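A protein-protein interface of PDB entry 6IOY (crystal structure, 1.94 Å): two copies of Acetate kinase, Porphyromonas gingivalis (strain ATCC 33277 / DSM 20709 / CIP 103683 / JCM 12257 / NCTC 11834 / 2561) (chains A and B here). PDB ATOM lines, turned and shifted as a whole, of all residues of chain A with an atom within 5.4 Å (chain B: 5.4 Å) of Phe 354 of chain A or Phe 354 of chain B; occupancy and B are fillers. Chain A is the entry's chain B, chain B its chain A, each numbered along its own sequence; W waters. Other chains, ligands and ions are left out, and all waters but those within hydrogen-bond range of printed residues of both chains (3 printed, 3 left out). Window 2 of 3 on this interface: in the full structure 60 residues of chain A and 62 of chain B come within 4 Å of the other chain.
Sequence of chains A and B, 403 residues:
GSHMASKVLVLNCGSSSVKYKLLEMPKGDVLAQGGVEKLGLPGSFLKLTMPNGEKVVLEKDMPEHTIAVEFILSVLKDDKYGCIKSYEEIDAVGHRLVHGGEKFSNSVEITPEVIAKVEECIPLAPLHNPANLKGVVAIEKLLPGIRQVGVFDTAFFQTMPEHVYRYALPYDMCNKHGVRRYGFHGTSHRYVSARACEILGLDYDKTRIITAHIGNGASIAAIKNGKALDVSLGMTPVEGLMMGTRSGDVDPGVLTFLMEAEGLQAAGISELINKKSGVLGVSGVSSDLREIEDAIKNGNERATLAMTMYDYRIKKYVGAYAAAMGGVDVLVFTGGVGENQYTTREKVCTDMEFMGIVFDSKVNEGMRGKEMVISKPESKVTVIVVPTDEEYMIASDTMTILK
Gly 319 of chain A touches Ala 323 of chain B, and with the chains exchanged Ala 323 of chain A touches Gly 319 of chain B.
Ala 322 of chain A touches Phe 354 of chain B, and with the chains exchanged Phe 354 of chain A touches Ala 322 of chain B.
Ala 323 of chain A touches Met 352 of chain B, and with the chains exchanged Met 352 of chain A touches Ala 323 of chain B.
Phe 354 of chain B touches its own counterpart, Phe 354 of chain A.
13 positions are printed for both chains.
Of the 18 pairs that touch across the chains among the printed residues, 18 have their exchanged pair printed and touching as well.
Water W2 bridges the backbone carbonyl oxygen of Phe 354 of chain B (2.7 Å) and the side-chain amino group of Lys 380 of chain A (3.2 Å).
Water W3 lies within hydrogen-bond range of the backbone carbonyl oxygen (O) of Gly 326 of chain A (2.8 Å), the backbone NH (N) of Phe 354 of chain B (3.0 Å) and the side-chain carboxylate (OE1) of Glu 353 of chain B (3.1 Å).
Water W1 bridges the side-chain amino group of Lys 380 of chain A and the backbone NH of Phe 354 of chain B.
Gly 319 of chain B touches Gly 319 of chain A (CA to O, 3.4 Å).
CA of Gly 319 of chain A touches CB of Ala 323 of chain B, at 3.8 Å.
Phe 354 of chain B touches Ala 322 of chain A.
SD of Met 352 of chain B touches CB of Ala 323 of chain A, at 3.9 Å.
Gly 327 of chain A touches Phe 354 of chain B (N to CD1, 3.6 Å).
SD of Met 352 of chain A touches CB of Ala 323 of chain B (3.9 Å).
Phe 354 of chain A touches Ala 322 of chain B.
CD1 of Phe 354 of chain A touches C of Gly 326 of chain B (3.5 Å).
Phe 354 of chain A touches Gly 327 of chain B (CD1 to N, 3.5 Å).
O of Phe 354 of chain B touches CA of Met 355 of chain A, at 3.6 Å.
O of Ala 322 of chain B sits at hydrogen-bond distance from N of Gly 327 of chain B, at 2.8 Å.
The backbone carbonyl oxygen (O) of Ala 322 of chain A is in hydrogen-bond range of the backbone NH (N) of Gly 327 of chain A (2.8 Å).
Hydrophobic or aromatic side chains of chain B within 4 Å of the printed part of chain A: Ala 322, Ala 323, Met 352, Phe 354 and Met 355.
Of the 13 printed residues of chain A, 9 touch a printed residue of chain B.
Printed residues of chain A that touch a printed residue of chain B: Gly 319, Ala 322, Ala 323, Gly 326, Gly 327, Asp 351, Met 352, Phe 354 and Met 355.
Hydrophobic or aromatic side chains of chain A that line the printed part of chain B: Ala 322, Ala 323, Met 352 and Phe 354.
Along chain A the printed residues that touch a printed residue of chain B span positions 319 to 355.
Among the printed residues, 18 pairs touch across the chains.
The backbone carbonyl oxygen of Phe 354 of chain B sits close to the backbone carbonyl oxygen of Phe 354 of chain A, 3.2 Å away.
Printed residues of chain B within 4 Å of Asp 351 of chain A: Gly 326 (3.2 Å).
Of chain B, only Ala 322 (3.5 Å), Ala 323 (3.4 Å), Gly 326 (3.5 Å), Gly 327 (3.5 Å), Phe 354 (3.2 Å) and Met 355 (3.5 Å) come within 4 Å of Phe 354 of chain A.
Lys 380 of chain A touches none of the printed residues of chain B.
Of the printed residues of chain A, Gly 319 of chain B touches Gly 319 and Ala 323.
Printed residues of chain A within 4 Å of Ala 323 of chain B: Gly 319, Met 352 and Phe 354.
Val 328 of chain B touches none of the printed residues of chain A.
Printed residues of chain A within 4 Å of Phe 354 of chain B: Ala 322 (3.6 Å), Ala 323 (3.6 Å), Gly 326 (3.6 Å), Gly 327 (3.6 Å), Phe 354 (3.2 Å) and Met 355 (3.6 Å).
The nearest printed residue of chain B that does not touch Ala 322 of chain A is Asp 351 of chain B (5.5 Å).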
ATOM      1  N   GLY A 319      -7.047  18.111 -16.036  1.00  0.00           N
ATOM      2  CA  GLY A 319      -6.178  17.579 -17.063  1.00  0.00           C
ATOM      3  C   GLY A 319      -5.198  18.600 -17.602  1.00  0.00           C
ATOM      4  O   GLY A 319      -4.020  18.288 -17.784  1.00  0.00           O
ATOM      5  N   ALA A 322      -2.467  19.488 -14.975  1.00  0.00           N
ATOM      6  CA  ALA A 322      -1.491  18.368 -14.849  1.00  0.00           C
ATOM      7  C   ALA A 322      -0.520  18.422 -16.042  1.00  0.00           C
ATOM      8  O   ALA A 322       0.698  18.344 -15.852  1.00  0.00           O
ATOM      9  CB  ALA A 322      -2.199  17.050 -14.750  1.00  0.00           C
ATOM     10  N   ALA A 323      -1.049  18.644 -17.250  1.00  0.00           N
ATOM     11  CA  ALA A 323      -0.212  18.743 -18.437  1.00  0.00           C
ATOM     12  C   ALA A 323       0.721  19.945 -18.304  1.00  0.00           C
ATOM     13  O   ALA A 323       1.887  19.828 -18.605  1.00  0.00           O
ATOM     14  CB  ALA A 323      -1.033  18.822 -19.709  1.00  0.00           C
ATOM     15  N   GLY A 326       3.563  18.940 -16.031  1.00  0.00           N
ATOM     16  CA  GLY A 326       4.264  17.685 -16.307  1.00  0.00           C
ATOM     17  C   GLY A 326       3.859  16.556 -15.371  1.00  0.00           C
ATOM     18  O   GLY A 326       4.654  15.572 -15.193  1.00  0.00           O
ATOM     19  N   GLY A 327       2.691  16.687 -14.751  1.00  0.00           N
ATOM     20  CA  GLY A 327       2.133  15.712 -13.819  1.00  0.00           C
ATOM     21  C   GLY A 327       1.537  16.434 -12.610  1.00  0.00           C
ATOM     22  O   GLY A 327       1.546  17.667 -12.540  1.00  0.00           O
ATOM     23  N   VAL A 328       0.944  15.665 -11.695  1.00  0.00           N
ATOM     24  CA  VAL A 328       0.352  16.211 -10.511  1.00  0.00           C
ATOM     25  C   VAL A 328       0.556  15.208  -9.378  1.00  0.00           C
ATOM     26  O   VAL A 328       0.408  14.007  -9.578  1.00  0.00           O
ATOM     27  CB  VAL A 328      -1.136  16.564 -10.704  1.00  0.00           C
ATOM     28  CG1 VAL A 328      -1.966  15.381 -11.191  1.00  0.00           C
ATOM     29  CG2 VAL A 328      -1.718  17.145  -9.454  1.00  0.00           C
ATOM     30  N   ASP A 351     -12.807   8.071 -13.763  1.00  0.00           N
ATOM     31  CA  ASP A 351     -12.271   7.890 -15.114  1.00  0.00           C
ATOM     32  C   ASP A 351     -11.066   8.822 -15.360  1.00  0.00           C
ATOM     33  O   ASP A 351     -10.949   9.493 -16.438  1.00  0.00           O
ATOM     34  CB  ASP A 351     -13.331   8.149 -16.180  1.00  0.00           C
ATOM     35  CG  ASP A 351     -13.032   7.364 -17.453  1.00  0.00           C
ATOM     36  OD1 ASP A 351     -12.118   6.479 -17.408  1.00  0.00           O
ATOM     37  OD2 ASP A 351     -13.713   7.639 -18.514  1.00  0.00           O
ATOM     38  N   MET A 352     -10.197   8.915 -14.356  1.00  0.00           N
ATOM     39  CA  MET A 352      -8.993   9.698 -14.436  1.00  0.00           C
ATOM     40  C   MET A 352      -7.793   8.831 -14.057  1.00  0.00           C
ATOM     41  O   MET A 352      -6.712   9.363 -13.774  1.00  0.00           O
ATOM     42  CB  MET A 352      -9.080  10.915 -13.503  1.00  0.00           C
ATOM     43  CG  MET A 352     -10.240  11.830 -13.816  1.00  0.00           C
ATOM     44  SD  MET A 352      -9.888  12.889 -15.202  1.00  0.00           S
ATOM     45  CE  MET A 352      -9.122  14.291 -14.356  1.00  0.00           C
ATOM     46  N   GLU A 353      -7.948   7.501 -14.163  1.00  0.00           N
ATOM     47  CA  GLU A 353      -6.824   6.580 -13.857  1.00  0.00           C
ATOM     48  C   GLU A 353      -5.664   6.797 -14.845  1.00  0.00           C
ATOM     49  O   GLU A 353      -4.511   6.539 -14.481  1.00  0.00           O
ATOM     50  CB  GLU A 353      -7.248   5.114 -13.929  1.00  0.00           C
ATOM     51  CG  GLU A 353      -8.356   4.756 -12.967  1.00  0.00           C
ATOM     52  CD  GLU A 353      -9.786   4.902 -13.469  1.00  0.00           C
ATOM     53  OE1 GLU A 353     -10.013   5.571 -14.499  1.00  0.00           O
ATOM     54  OE2 GLU A 353     -10.681   4.378 -12.774  1.00  0.00           O
ATOM     55  N   PHE A 354      -5.961   7.264 -16.069  1.00  0.00           N
ATOM     56  CA  PHE A 354      -4.914   7.496 -17.115  1.00  0.00           C
ATOM     57  C   PHE A 354      -3.865   8.502 -16.620  1.00  0.00           C
ATOM     58  O   PHE A 354      -2.734   8.511 -17.120  1.00  0.00           O
ATOM     59  CB  PHE A 354      -5.512   7.962 -18.456  1.00  0.00           C
ATOM     60  CG  PHE A 354      -5.929   9.412 -18.435  1.00  0.00           C
ATOM     61  CD1 PHE A 354      -7.139   9.794 -17.886  1.00  0.00           C
ATOM     62  CD2 PHE A 354      -5.059  10.409 -18.864  1.00  0.00           C
ATOM     63  CE1 PHE A 354      -7.485  11.134 -17.793  1.00  0.00           C
ATOM     64  CE2 PHE A 354      -5.410  11.751 -18.784  1.00  0.00           C
ATOM     65  CZ  PHE A 354      -6.626  12.116 -18.261  1.00  0.00           C
ATOM     66  N   MET A 355      -4.231   9.367 -15.665  1.00  0.00           N
ATOM     67  CA  MET A 355      -3.304  10.373 -15.163  1.00  0.00           C
ATOM     68  C   MET A 355      -3.004  10.159 -13.681  1.00  0.00           C
ATOM     69  O   MET A 355      -2.500  11.075 -13.019  1.00  0.00           O
ATOM     70  CB  MET A 355      -3.799  11.811 -15.413  1.00  0.00           C
ATOM     71  CG  MET A 355      -5.141  12.100 -14.835  1.00  0.00           C
ATOM     72  SD  MET A 355      -5.549  13.879 -15.045  1.00  0.00           S
ATOM     73  CE  MET A 355      -4.619  14.590 -13.699  1.00  0.00           C
ATOM     74  N   GLY A 356      -3.258   8.949 -13.173  1.00  0.00           N
ATOM     75  CA  GLY A 356      -2.842   8.543 -11.864  1.00  0.00           C
ATOM     76  C   GLY A 356      -3.849   8.710 -10.725  1.00  0.00           C
ATOM     77  O   GLY A 356      -3.476   8.525  -9.555  1.00  0.00           O
ATOM     78  N   LYS A 380      -1.831   6.974  -7.377  1.00  0.00           N
ATOM     79  CA  LYS A 380      -0.562   7.666  -7.537  1.00  0.00           C
ATOM     80  C   LYS A 380      -0.719   9.131  -7.096  1.00  0.00           C
ATOM     81  O   LYS A 380       0.116   9.666  -6.400  1.00  0.00           O
ATOM     82  CB  LYS A 380      -0.073   7.522  -8.976  1.00  0.00           C
ATOM     83  CG  LYS A 380       1.129   8.372  -9.333  1.00  0.00           C
ATOM     84  CD  LYS A 380       1.636   8.017 -10.699  1.00  0.00           C
ATOM     85  CE  LYS A 380       2.872   8.800 -11.081  1.00  0.00           C
ATOM     86  NZ  LYS A 380       3.191   8.547 -12.509  1.00  0.00           N
ATOM     87  N   GLY B 319      -3.954  17.814 -22.325  1.00  0.00           N
ATOM     88  CA  GLY B 319      -4.332  17.367 -20.992  1.00  0.00           C
ATOM     89  C   GLY B 319      -5.824  17.398 -20.745  1.00  0.00           C
ATOM     90  O   GLY B 319      -6.381  16.447 -20.232  1.00  0.00           O
ATOM     91  N   ALA B 322      -7.679  14.712 -22.906  1.00  0.00           N
ATOM     92  CA  ALA B 322      -7.461  13.362 -22.326  1.00  0.00           C
ATOM     93  C   ALA B 322      -8.376  13.178 -21.104  1.00  0.00           C
ATOM     94  O   ALA B 322      -9.060  12.136 -20.984  1.00  0.00           O
ATOM     95  CB  ALA B 322      -6.017  13.169 -22.012  1.00  0.00           C
ATOM     96  N   ALA B 323      -8.441  14.202 -20.242  1.00  0.00           N
ATOM     97  CA  ALA B 323      -9.300  14.141 -19.070  1.00  0.00           C
ATOM     98  C   ALA B 323     -10.770  14.002 -19.498  1.00  0.00           C
ATOM     99  O   ALA B 323     -11.492  13.212 -18.949  1.00  0.00           O
ATOM    100  CB  ALA B 323      -9.061  15.295 -18.145  1.00  0.00           C
ATOM    101  N   GLY B 326     -11.349  10.401 -20.533  1.00  0.00           N
ATOM    102  CA  GLY B 326     -10.936   9.346 -19.620  1.00  0.00           C
ATOM    103  C   GLY B 326      -9.667   8.642 -20.060  1.00  0.00           C
ATOM    104  O   GLY B 326      -9.371   7.559 -19.577  1.00  0.00           O
ATOM    105  N   GLY B 327      -8.868   9.309 -20.902  1.00  0.00           N
ATOM    106  CA  GLY B 327      -7.628   8.791 -21.449  1.00  0.00           C
ATOM    107  C   GLY B 327      -7.531   9.112 -22.938  1.00  0.00           C
ATOM    108  O   GLY B 327      -8.445   9.668 -23.487  1.00  0.00           O
ATOM    109  N   VAL B 328      -6.389   8.799 -23.545  1.00  0.00           N
ATOM    110  CA  VAL B 328      -6.127   9.000 -24.947  1.00  0.00           C
ATOM    111  C   VAL B 328      -5.260   7.847 -25.449  1.00  0.00           C
ATOM    112  O   VAL B 328      -4.365   7.400 -24.756  1.00  0.00           O
ATOM    113  CB  VAL B 328      -5.480  10.372 -25.221  1.00  0.00           C
ATOM    114  CG1 VAL B 328      -4.192  10.597 -24.465  1.00  0.00           C
ATOM    115  CG2 VAL B 328      -5.209  10.555 -26.703  1.00  0.00           C
ATOM    116  N   ASP B 351       7.515  15.790 -21.176  1.00  0.00           N
ATOM    117  CA  ASP B 351       6.998  15.855 -19.794  1.00  0.00           C
ATOM    118  C   ASP B 351       5.495  15.559 -19.748  1.00  0.00           C
ATOM    119  O   ASP B 351       4.696  16.274 -19.075  1.00  0.00           O
ATOM    120  CB  ASP B 351       7.303  17.204 -19.157  1.00  0.00           C
ATOM    121  CG  ASP B 351       8.772  17.521 -19.177  1.00  0.00           C
ATOM    122  OD1 ASP B 351       9.575  16.650 -18.718  1.00  0.00           O
ATOM    123  OD2 ASP B 351       9.126  18.546 -19.751  1.00  0.00           O
ATOM    124  N   MET B 352       5.091  14.558 -20.529  1.00  0.00           N
ATOM    125  CA  MET B 352       3.724  14.089 -20.571  1.00  0.00           C
ATOM    126  C   MET B 352       3.671  12.589 -20.263  1.00  0.00           C
ATOM    127  O   MET B 352       2.649  11.934 -20.538  1.00  0.00           O
ATOM    128  CB  MET B 352       3.099  14.405 -21.927  1.00  0.00           C
ATOM    129  CG  MET B 352       3.119  15.867 -22.262  1.00  0.00           C
ATOM    130  SD  MET B 352       1.798  16.785 -21.467  1.00  0.00           S
ATOM    131  CE  MET B 352       0.501  16.597 -22.677  1.00  0.00           C
ATOM    132  N   GLU B 353       4.722  12.057 -19.625  1.00  0.00           N
ATOM    133  CA  GLU B 353       4.764  10.610 -19.298  1.00  0.00           C
ATOM    134  C   GLU B 353       3.643  10.236 -18.338  1.00  0.00           C
ATOM    135  O   GLU B 353       3.166   9.116 -18.385  1.00  0.00           O
ATOM    136  CB  GLU B 353       6.103  10.197 -18.656  1.00  0.00           C
ATOM    137  CG  GLU B 353       7.299  10.440 -19.552  1.00  0.00           C
ATOM    138  CD  GLU B 353       7.951  11.806 -19.478  1.00  0.00           C
ATOM    139  OE1 GLU B 353       7.392  12.743 -18.870  1.00  0.00           O
ATOM    140  OE2 GLU B 353       9.023  11.943 -20.099  1.00  0.00           O
ATOM    141  N   PHE B 354       3.259  11.176 -17.455  1.00  0.00           N
ATOM    142  CA  PHE B 354       2.201  10.955 -16.438  1.00  0.00           C
ATOM    143  C   PHE B 354       0.889  10.512 -17.100  1.00  0.00           C
ATOM    144  O   PHE B 354       0.066   9.883 -16.426  1.00  0.00           O
ATOM    145  CB  PHE B 354       1.956  12.207 -15.578  1.00  0.00           C
ATOM    146  CG  PHE B 354       1.186  13.283 -16.278  1.00  0.00           C
ATOM    147  CD1 PHE B 354       1.819  14.165 -17.140  1.00  0.00           C
ATOM    148  CD2 PHE B 354      -0.185  13.372 -16.144  1.00  0.00           C
ATOM    149  CE1 PHE B 354       1.088  15.117 -17.842  1.00  0.00           C
ATOM    150  CE2 PHE B 354      -0.915  14.336 -16.823  1.00  0.00           C
ATOM    151  CZ  PHE B 354      -0.274  15.201 -17.674  1.00  0.00           C
ATOM    152  N   MET B 355       0.669  10.871 -18.380  1.00  0.00           N
ATOM    153  CA  MET B 355      -0.577  10.516 -19.049  1.00  0.00           C
ATOM    154  C   MET B 355      -0.320   9.580 -20.234  1.00  0.00           C
ATOM    155  O   MET B 355      -1.179   9.413 -21.089  1.00  0.00           O
ATOM    156  CB  MET B 355      -1.352  11.761 -19.519  1.00  0.00           C
ATOM    157  CG  MET B 355      -0.528  12.687 -20.404  1.00  0.00           C
ATOM    158  SD  MET B 355      -1.593  14.039 -21.112  1.00  0.00           S
ATOM    159  CE  MET B 355      -2.423  13.150 -22.415  1.00  0.00           C
ATOM    160  N   GLY B 356       0.842   8.931 -20.252  1.00  0.00           N
ATOM    161  CA  GLY B 356       1.119   7.816 -21.148  1.00  0.00           C
ATOM    162  C   GLY B 356       1.936   8.178 -22.390  1.00  0.00           C
ATOM    163  O   GLY B 356       2.104   7.294 -23.281  1.00  0.00           O
ATOM    164  N   LYS B 380       2.604   4.316 -24.242  1.00  0.00           N
ATOM    165  CA  LYS B 380       1.240   3.837 -24.162  1.00  0.00           C
ATOM    166  C   LYS B 380       0.364   4.590 -25.188  1.00  0.00           C
ATOM    167  O   LYS B 380      -0.453   3.999 -25.866  1.00  0.00           O
ATOM    168  CB  LYS B 380       0.693   3.996 -22.751  1.00  0.00           C
ATOM    169  CG  LYS B 380      -0.729   3.480 -22.609  1.00  0.00           C
ATOM    170  CD  LYS B 380      -1.371   3.826 -21.295  1.00  0.00           C
ATOM    171  CE  LYS B 380      -2.358   2.775 -20.812  1.00  0.00           C
ATOM    172  NZ  LYS B 380      -2.842   3.155 -19.463  1.00  0.00           N
HETATM  173  O   HOH W   1       4.885   9.050 -15.279  1.00  0.00           O
HETATM  174  O   HOH W   2       0.380   8.846 -13.993  1.00  0.00           O
HETATM  175  O   HOH W   3       5.259  13.254 -16.668  1.00  0.00           O
